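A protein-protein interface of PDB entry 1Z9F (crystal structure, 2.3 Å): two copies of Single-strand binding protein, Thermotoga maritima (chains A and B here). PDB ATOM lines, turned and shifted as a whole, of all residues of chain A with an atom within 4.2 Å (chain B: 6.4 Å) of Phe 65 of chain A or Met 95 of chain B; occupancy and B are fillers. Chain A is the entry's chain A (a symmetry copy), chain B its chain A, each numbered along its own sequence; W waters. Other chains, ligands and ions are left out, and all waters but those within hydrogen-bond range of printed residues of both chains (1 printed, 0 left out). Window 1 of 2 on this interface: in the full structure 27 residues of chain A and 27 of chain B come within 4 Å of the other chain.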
ATOM      1  N   LEU A  21     -19.461  26.270  -6.980  1.00  0.00           N
ATOM      2  CA  LEU A  21     -19.245  25.614  -8.273  1.00  0.00           C
ATOM      3  C   LEU A  21     -19.110  26.716  -9.284  1.00  0.00           C
ATOM      4  O   LEU A  21     -19.730  27.758  -9.122  1.00  0.00           O
ATOM      5  CB  LEU A  21     -20.451  24.744  -8.646  1.00  0.00           C
ATOM      6  CG  LEU A  21     -20.818  23.672  -7.614  1.00  0.00           C
ATOM      7  CD1 LEU A  21     -22.154  23.105  -7.869  1.00  0.00           C
ATOM      8  CD2 LEU A  21     -19.760  22.587  -7.562  1.00  0.00           C
ATOM      9  N   PHE A  43     -31.767  24.787 -13.061  1.00  0.00           N
ATOM     10  CA  PHE A  43     -30.885  24.564 -14.189  1.00  0.00           C
ATOM     11  C   PHE A  43     -29.732  23.698 -13.714  1.00  0.00           C
ATOM     12  O   PHE A  43     -29.461  23.610 -12.530  1.00  0.00           O
ATOM     13  CB  PHE A  43     -30.378  25.879 -14.791  1.00  0.00           C
ATOM     14  CG  PHE A  43     -29.694  26.782 -13.819  1.00  0.00           C
ATOM     15  CD1 PHE A  43     -30.428  27.638 -13.015  1.00  0.00           C
ATOM     16  CD2 PHE A  43     -28.310  26.821 -13.744  1.00  0.00           C
ATOM     17  CE1 PHE A  43     -29.797  28.509 -12.125  1.00  0.00           C
ATOM     18  CE2 PHE A  43     -27.657  27.686 -12.850  1.00  0.00           C
ATOM     19  CZ  PHE A  43     -28.409  28.531 -12.040  1.00  0.00           C
ATOM     20  N   THR A  44     -29.097  23.021 -14.652  1.00  0.00           N
ATOM     21  CA  THR A  44     -28.024  22.116 -14.349  1.00  0.00           C
ATOM     22  C   THR A  44     -26.816  22.687 -15.040  1.00  0.00           C
ATOM     23  O   THR A  44     -26.901  23.167 -16.178  1.00  0.00           O
ATOM     24  CB  THR A  44     -28.298  20.655 -14.819  1.00  0.00           C
ATOM     25  OG1 THR A  44     -27.788  20.453 -16.145  1.00  0.00           O
ATOM     26  CG2 THR A  44     -29.815  20.312 -14.769  1.00  0.00           C
ATOM     27  N   ILE A  45     -25.696  22.669 -14.318  1.00  0.00           N
ATOM     28  CA  ILE A  45     -24.441  23.170 -14.840  1.00  0.00           C
ATOM     29  C   ILE A  45     -23.473  22.015 -15.083  1.00  0.00           C
ATOM     30  O   ILE A  45     -23.566  20.958 -14.443  1.00  0.00           O
ATOM     31  CB  ILE A  45     -23.822  24.252 -13.920  1.00  0.00           C
ATOM     32  CG1 ILE A  45     -23.692  23.748 -12.476  1.00  0.00           C
ATOM     33  CG2 ILE A  45     -24.675  25.531 -13.985  1.00  0.00           C
ATOM     34  CD1 ILE A  45     -22.935  24.688 -11.576  1.00  0.00           C
ATOM     35  N   VAL A  47     -19.768  21.065 -14.669  1.00  0.00           N
ATOM     36  CA  VAL A  47     -18.552  21.451 -13.952  1.00  0.00           C
ATOM     37  C   VAL A  47     -17.489  20.404 -14.228  1.00  0.00           C
ATOM     38  O   VAL A  47     -17.361  19.412 -13.495  1.00  0.00           O
ATOM     39  CB  VAL A  47     -18.798  21.531 -12.420  1.00  0.00           C
ATOM     40  CG1 VAL A  47     -17.488  21.862 -11.655  1.00  0.00           C
ATOM     41  CG2 VAL A  47     -19.919  22.545 -12.091  1.00  0.00           C
ATOM     42  N   ASP A  63     -18.837  16.668 -13.987  1.00  0.00           N
ATOM     43  CA  ASP A  63     -19.849  16.513 -12.962  1.00  0.00           C
ATOM     44  C   ASP A  63     -20.996  17.450 -13.271  1.00  0.00           C
ATOM     45  O   ASP A  63     -20.790  18.650 -13.487  1.00  0.00           O
ATOM     46  CB  ASP A  63     -19.278  16.866 -11.599  1.00  0.00           C
ATOM     47  CG  ASP A  63     -18.359  15.816 -11.082  1.00  0.00           C
ATOM     48  OD1 ASP A  63     -18.824  14.671 -10.928  1.00  0.00           O
ATOM     49  OD2 ASP A  63     -17.181  16.127 -10.826  1.00  0.00           O
ATOM     50  N   PHE A  64     -22.206  16.900 -13.280  1.00  0.00           N
ATOM     51  CA  PHE A  64     -23.413  17.678 -13.525  1.00  0.00           C
ATOM     52  C   PHE A  64     -24.164  17.908 -12.223  1.00  0.00           C
ATOM     53  O   PHE A  64     -24.307  16.998 -11.401  1.00  0.00           O
ATOM     54  CB  PHE A  64     -24.297  16.972 -14.552  1.00  0.00           C
ATOM     55  CG  PHE A  64     -23.717  16.974 -15.934  1.00  0.00           C
ATOM     56  CD1 PHE A  64     -23.968  18.032 -16.799  1.00  0.00           C
ATOM     57  CD2 PHE A  64     -22.903  15.940 -16.366  1.00  0.00           C
ATOM     58  CE1 PHE A  64     -23.426  18.051 -18.075  1.00  0.00           C
ATOM     59  CE2 PHE A  64     -22.356  15.956 -17.650  1.00  0.00           C
ATOM     60  CZ  PHE A  64     -22.618  17.010 -18.503  1.00  0.00           C
ATOM     61  N   PHE A  65     -24.630  19.139 -12.045  1.00  0.00           N
ATOM     62  CA  PHE A  65     -25.320  19.542 -10.831  1.00  0.00           C
ATOM     63  C   PHE A  65     -26.649  20.227 -11.145  1.00  0.00           C
ATOM     64  O   PHE A  65     -26.677  21.218 -11.868  1.00  0.00           O
ATOM     65  CB  PHE A  65     -24.433  20.521 -10.039  1.00  0.00           C
ATOM     66  CG  PHE A  65     -23.113  19.926  -9.597  1.00  0.00           C
ATOM     67  CD1 PHE A  65     -21.999  20.016 -10.399  1.00  0.00           C
ATOM     68  CD2 PHE A  65     -23.000  19.297  -8.370  1.00  0.00           C
ATOM     69  CE1 PHE A  65     -20.820  19.477 -10.006  1.00  0.00           C
ATOM     70  CE2 PHE A  65     -21.815  18.770  -7.966  1.00  0.00           C
ATOM     71  CZ  PHE A  65     -20.724  18.842  -8.786  1.00  0.00           C
ATOM     72  N   ARG A  66     -27.737  19.715 -10.585  1.00  0.00           N
ATOM     73  CA  ARG A  66     -29.021  20.437 -10.594  1.00  0.00           C
ATOM     74  C   ARG A  66     -28.950  21.641  -9.647  1.00  0.00           C
ATOM     75  O   ARG A  66     -28.783  21.448  -8.447  1.00  0.00           O
ATOM     76  CB  ARG A  66     -30.157  19.502 -10.155  1.00  0.00           C
ATOM     77  CG  ARG A  66     -31.549  20.144 -10.195  1.00  0.00           C
ATOM     78  CD  ARG A  66     -32.657  19.104 -10.172  1.00  0.00           C
ATOM     79  N   ILE A  67     -29.038  22.866 -10.188  1.00  0.00           N
ATOM     80  CA  ILE A  67     -29.127  24.107  -9.389  1.00  0.00           C
ATOM     81  C   ILE A  67     -30.600  24.562  -9.211  1.00  0.00           C
ATOM     82  O   ILE A  67     -31.352  24.669 -10.176  1.00  0.00           O
ATOM     83  CB  ILE A  67     -28.343  25.301 -10.043  1.00  0.00           C
ATOM     84  CG1 ILE A  67     -26.931  24.910 -10.526  1.00  0.00           C
ATOM     85  CG2 ILE A  67     -28.263  26.497  -9.094  1.00  0.00           C
ATOM     86  CD1 ILE A  67     -26.097  24.213  -9.520  1.00  0.00           C
ATOM     87  N   ASN B  17     -14.953  23.542  -8.223  1.00  0.00           N
ATOM     88  CA  ASN B  17     -15.836  22.624  -7.526  1.00  0.00           C
ATOM     89  C   ASN B  17     -15.318  22.488  -6.117  1.00  0.00           C
ATOM     90  O   ASN B  17     -14.297  21.909  -5.916  1.00  0.00           O
ATOM     91  CB  ASN B  17     -15.842  21.283  -8.256  1.00  0.00           C
ATOM     92  CG  ASN B  17     -16.637  20.222  -7.552  1.00  0.00           C
ATOM     93  OD1 ASN B  17     -16.790  20.235  -6.334  1.00  0.00           O
ATOM     94  ND2 ASN B  17     -17.127  19.249  -8.332  1.00  0.00           N
ATOM     95  N   MET B  93     -17.253  17.835  -4.864  1.00  0.00           N
ATOM     96  CA  MET B  93     -18.507  17.110  -4.961  1.00  0.00           C
ATOM     97  C   MET B  93     -18.460  16.383  -6.292  1.00  0.00           C
ATOM     98  O   MET B  93     -18.511  17.000  -7.354  1.00  0.00           O
ATOM     99  CB  MET B  93     -19.692  18.065  -4.835  1.00  0.00           C
ATOM    100  CG  MET B  93     -21.069  17.372  -4.706  1.00  0.00           C
ATOM    101  SD  MET B  93     -21.209  16.228  -3.311  1.00  0.00           S
ATOM    102  CE  MET B  93     -21.235  14.691  -4.107  1.00  0.00           C
ATOM    103  N   ARG B  94     -18.275  15.067  -6.216  1.00  0.00           N
ATOM    104  CA  ARG B  94     -18.347  14.203  -7.403  1.00  0.00           C
ATOM    105  C   ARG B  94     -19.753  13.676  -7.661  1.00  0.00           C
ATOM    106  O   ARG B  94     -20.425  13.159  -6.772  1.00  0.00           O
ATOM    107  CB  ARG B  94     -17.370  13.026  -7.322  1.00  0.00           C
ATOM    108  CG  ARG B  94     -15.882  13.390  -7.366  1.00  0.00           C
ATOM    109  CD  ARG B  94     -15.567  14.610  -8.238  1.00  0.00           C
ATOM    110  NE  ARG B  94     -14.126  14.705  -8.544  1.00  0.00           N
ATOM    111  CZ  ARG B  94     -13.506  15.803  -9.001  1.00  0.00           C
ATOM    112  NH1 ARG B  94     -14.175  16.947  -9.199  1.00  0.00           N
ATOM    113  NH2 ARG B  94     -12.198  15.767  -9.250  1.00  0.00           N
ATOM    114  N   MET B  95     -20.159  13.805  -8.916  1.00  0.00           N
ATOM    115  CA  MET B  95     -21.464  13.387  -9.398  1.00  0.00           C
ATOM    116  C   MET B  95     -21.265  12.192 -10.324  1.00  0.00           C
ATOM    117  O   MET B  95     -21.409  12.297 -11.541  1.00  0.00           O
ATOM    118  CB  MET B  95     -22.101  14.555 -10.151  1.00  0.00           C
ATOM    119  CG  MET B  95     -22.448  15.718  -9.259  1.00  0.00           C
ATOM    120  SD  MET B  95     -23.942  15.315  -8.321  1.00  0.00           S
ATOM    121  CE  MET B  95     -23.203  15.032  -6.736  1.00  0.00           C
ATOM    122  N   ARG B  96     -20.902  11.064  -9.729  1.00  0.00           N
ATOM    123  CA  ARG B  96     -20.334   9.974 -10.503  1.00  0.00           C
ATOM    124  C   ARG B  96     -21.447   9.094 -11.056  1.00  0.00           C
ATOM    125  O   ARG B  96     -22.290   8.583 -10.318  1.00  0.00           O
ATOM    126  CB  ARG B  96     -19.292   9.179  -9.696  1.00  0.00           C
ATOM    127  CG  ARG B  96     -19.668   7.752  -9.373  1.00  0.00           C
ATOM    128  CD  ARG B  96     -18.471   6.897  -8.973  1.00  0.00           C
ATOM    129  NE  ARG B  96     -18.884   5.894  -7.999  1.00  0.00           N
ATOM    130  CZ  ARG B  96     -19.678   4.863  -8.263  1.00  0.00           C
ATOM    131  NH1 ARG B  96     -20.137   4.628  -9.496  1.00  0.00           N
ATOM    132  NH2 ARG B  96     -19.993   4.024  -7.283  1.00  0.00           N
ATOM    133  N   ARG B  97     -21.436   8.943 -12.372  1.00  0.00           N
ATOM    134  CA  ARG B  97     -22.448   8.178 -13.082  1.00  0.00           C
ATOM    135  C   ARG B  97     -21.923   6.763 -13.280  1.00  0.00           C
ATOM    136  O   ARG B  97     -20.743   6.566 -13.577  1.00  0.00           O
ATOM    137  CB  ARG B  97     -22.765   8.838 -14.429  1.00  0.00           C
ATOM    138  CG  ARG B  97     -22.629  10.360 -14.439  1.00  0.00           C
ATOM    139  CD  ARG B  97     -22.980  10.947 -15.793  1.00  0.00           C
ATOM    140  NE  ARG B  97     -22.183  12.139 -16.057  1.00  0.00           N
ATOM    141  CZ  ARG B  97     -20.960  12.145 -16.588  1.00  0.00           C
ATOM    142  NH1 ARG B  97     -20.359  11.017 -16.950  1.00  0.00           N
ATOM    143  NH2 ARG B  97     -20.330  13.299 -16.764  1.00  0.00           N
ATOM    144  N   VAL B 107     -26.318   8.228 -11.371  1.00  0.00           N
ATOM    145  CA  VAL B 107     -25.479   9.266 -10.687  1.00  0.00           C
ATOM    146  C   VAL B 107     -25.345   9.171  -9.148  1.00  0.00           C
ATOM    147  O   VAL B 107     -26.327   9.409  -8.388  1.00  0.00           O
ATOM    148  CB  VAL B 107     -25.939  10.715 -11.046  1.00  0.00           C
ATOM    149  CG1 VAL B 107     -25.001  11.757 -10.430  1.00  0.00           C
ATOM    150  CG2 VAL B 107     -26.018  10.903 -12.566  1.00  0.00           C
ATOM    151  N   SER B 108     -24.109   8.884  -8.697  1.00  0.00           N
ATOM    152  CA  SER B 108     -23.816   8.691  -7.274  1.00  0.00           C
ATOM    153  C   SER B 108     -22.922   9.801  -6.689  1.00  0.00           C
ATOM    154  O   SER B 108     -21.766   9.939  -7.109  1.00  0.00           O
ATOM    155  CB  SER B 108     -23.122   7.355  -7.057  1.00  0.00           C
ATOM    156  OG  SER B 108     -22.567   7.307  -5.750  1.00  0.00           O
ATOM    157  N   PRO B 109     -23.443  10.558  -5.695  1.00  0.00           N
ATOM    158  CA  PRO B 109     -22.775  11.741  -5.127  1.00  0.00           C
ATOM    159  C   PRO B 109     -21.796  11.388  -4.022  1.00  0.00           C
ATOM    160  O   PRO B 109     -22.220  10.909  -2.977  1.00  0.00           O
ATOM    161  CB  PRO B 109     -23.949  12.557  -4.534  1.00  0.00           C
ATOM    162  CG  PRO B 109     -25.177  11.667  -4.671  1.00  0.00           C
ATOM    163  CD  PRO B 109     -24.720  10.312  -5.009  1.00  0.00           C
ATOM    164  N   GLU B 110     -20.505  11.614  -4.245  1.00  0.00           N
ATOM    165  CA  GLU B 110     -19.503  11.440  -3.185  1.00  0.00           C
ATOM    166  C   GLU B 110     -18.655  12.686  -3.050  1.00  0.00           C
ATOM    167  O   GLU B 110     -18.381  13.345  -4.052  1.00  0.00           O
ATOM    168  CB  GLU B 110     -18.505  10.340  -3.516  1.00  0.00           C
ATOM    169  CG  GLU B 110     -19.055   9.031  -3.951  1.00  0.00           C
ATOM    170  CD  GLU B 110     -18.069   8.297  -4.822  1.00  0.00           C
ATOM    171  OE1 GLU B 110     -16.887   8.768  -4.861  1.00  0.00           O
ATOM    172  OE2 GLU B 110     -18.476   7.296  -5.460  1.00  0.00           O
HETATM  173  O   HOH W   1     -22.238  14.008 -13.517  1.00  0.00           O
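Water W1 lies within hydrogen-bond range of O of Met 95 of chain B, N of Phe 64 of chain A and NE of Arg 97 of chain B.
Of the 10 printed residues of chain B, 5 touch a printed residue of chain A. Printed residues of chain B that touch a printed residue of chain A: Asn 17, Met 93, Arg 94, Met 95 and Arg 97. Along chain A the printed residues that touch a printed residue of chain B span positions 21 to 65. Among the printed residues, 11 pairs touch across the chains.
No position is printed for both chains.
CG of Asn 17 of chain B touches CD2 of Leu 21 of chain A (3.9 Å). CB of Asn 17 of chain B touches CG1 of Val 47 of chain A, 3.8 Å away. Asn 17 of chain B touches Asp 63 of chain A (ND2 to OD2, 3.996 Å). O of Met 93 of chain B touches OD2 of Asp 63 of chain A, 3.8 Å away. Phe 64 of chain A touches Arg 97 of chain B. Phe 65 of chain A touches Asn 17 of chain B. Phe 65 of chain A touches Met 93 of chain B. Met 95 of chain B touches Phe 65 of chain A (CG to CE2, 3.4 Å).
The backbone carbonyl oxygen (O) of Met 93 of chain B sits at hydrogen-bond distance from the side-chain amide nitrogen (ND2) of Asn 17 of chain B (2.8 Å). N of Arg 94 of chain B is in hydrogen-bond range of O of Glu 110 of chain B, 2.8 Å away. The backbone carbonyl oxygen (O) of Phe 65 of chain A sits at hydrogen-bond distance from the backbone NH (N) of Ile 45 of chain A, at 3.0 Å. O of Asp 63 of chain A lies within hydrogen-bond range of N of Val 47 of chain A, 2.9 Å away.
Printed residues of chain B within 4 Å of Leu 21 of chain A: Asn 17 (3.9 Å). Of chain B, only Asn 17 (3.6 Å), Met 93 (3.2 Å) and Met 95 (3.4 Å) come within 4 Å of Phe 65 of chain A. Of the printed residues of chain A, Met 93 of chain B touches Asp 63 (3.8 Å) and Phe 65 (3.2 Å). Printed residues of chain A within 4 Å of Arg 94 of chain B: Asp 63. Met 95 of chain B touches just these residues of chain A: Asp 63, Phe 64 and Phe 65. Of the printed residues of chain A, Arg 97 of chain B touches Phe 64 (3.5 Å). The nearest residue of chain B that does not touch Phe 65 of chain A is Arg 94 of chain B (5.2 Å). The nearest printed residue of chain B that does not touch Asp 63 of chain A is Arg 96 of chain B (4.3 Å).
The guanidinium group (NH1) of Arg 94 of chain B lies within salt-bridge range of the side-chain carboxylate (OD2) of Asp 63 of chain A (3.5 Å). The backbone NH (N) of Met 95 of chain B is in hydrogen-bond range of the side-chain carboxylate (OD1) of Asp 63 of chain A. The backbone carbonyl oxygen (O) of Phe 64 of chain A lies close to the side-chain sulfur (SD) of Met 95 of chain B (3.5 Å).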
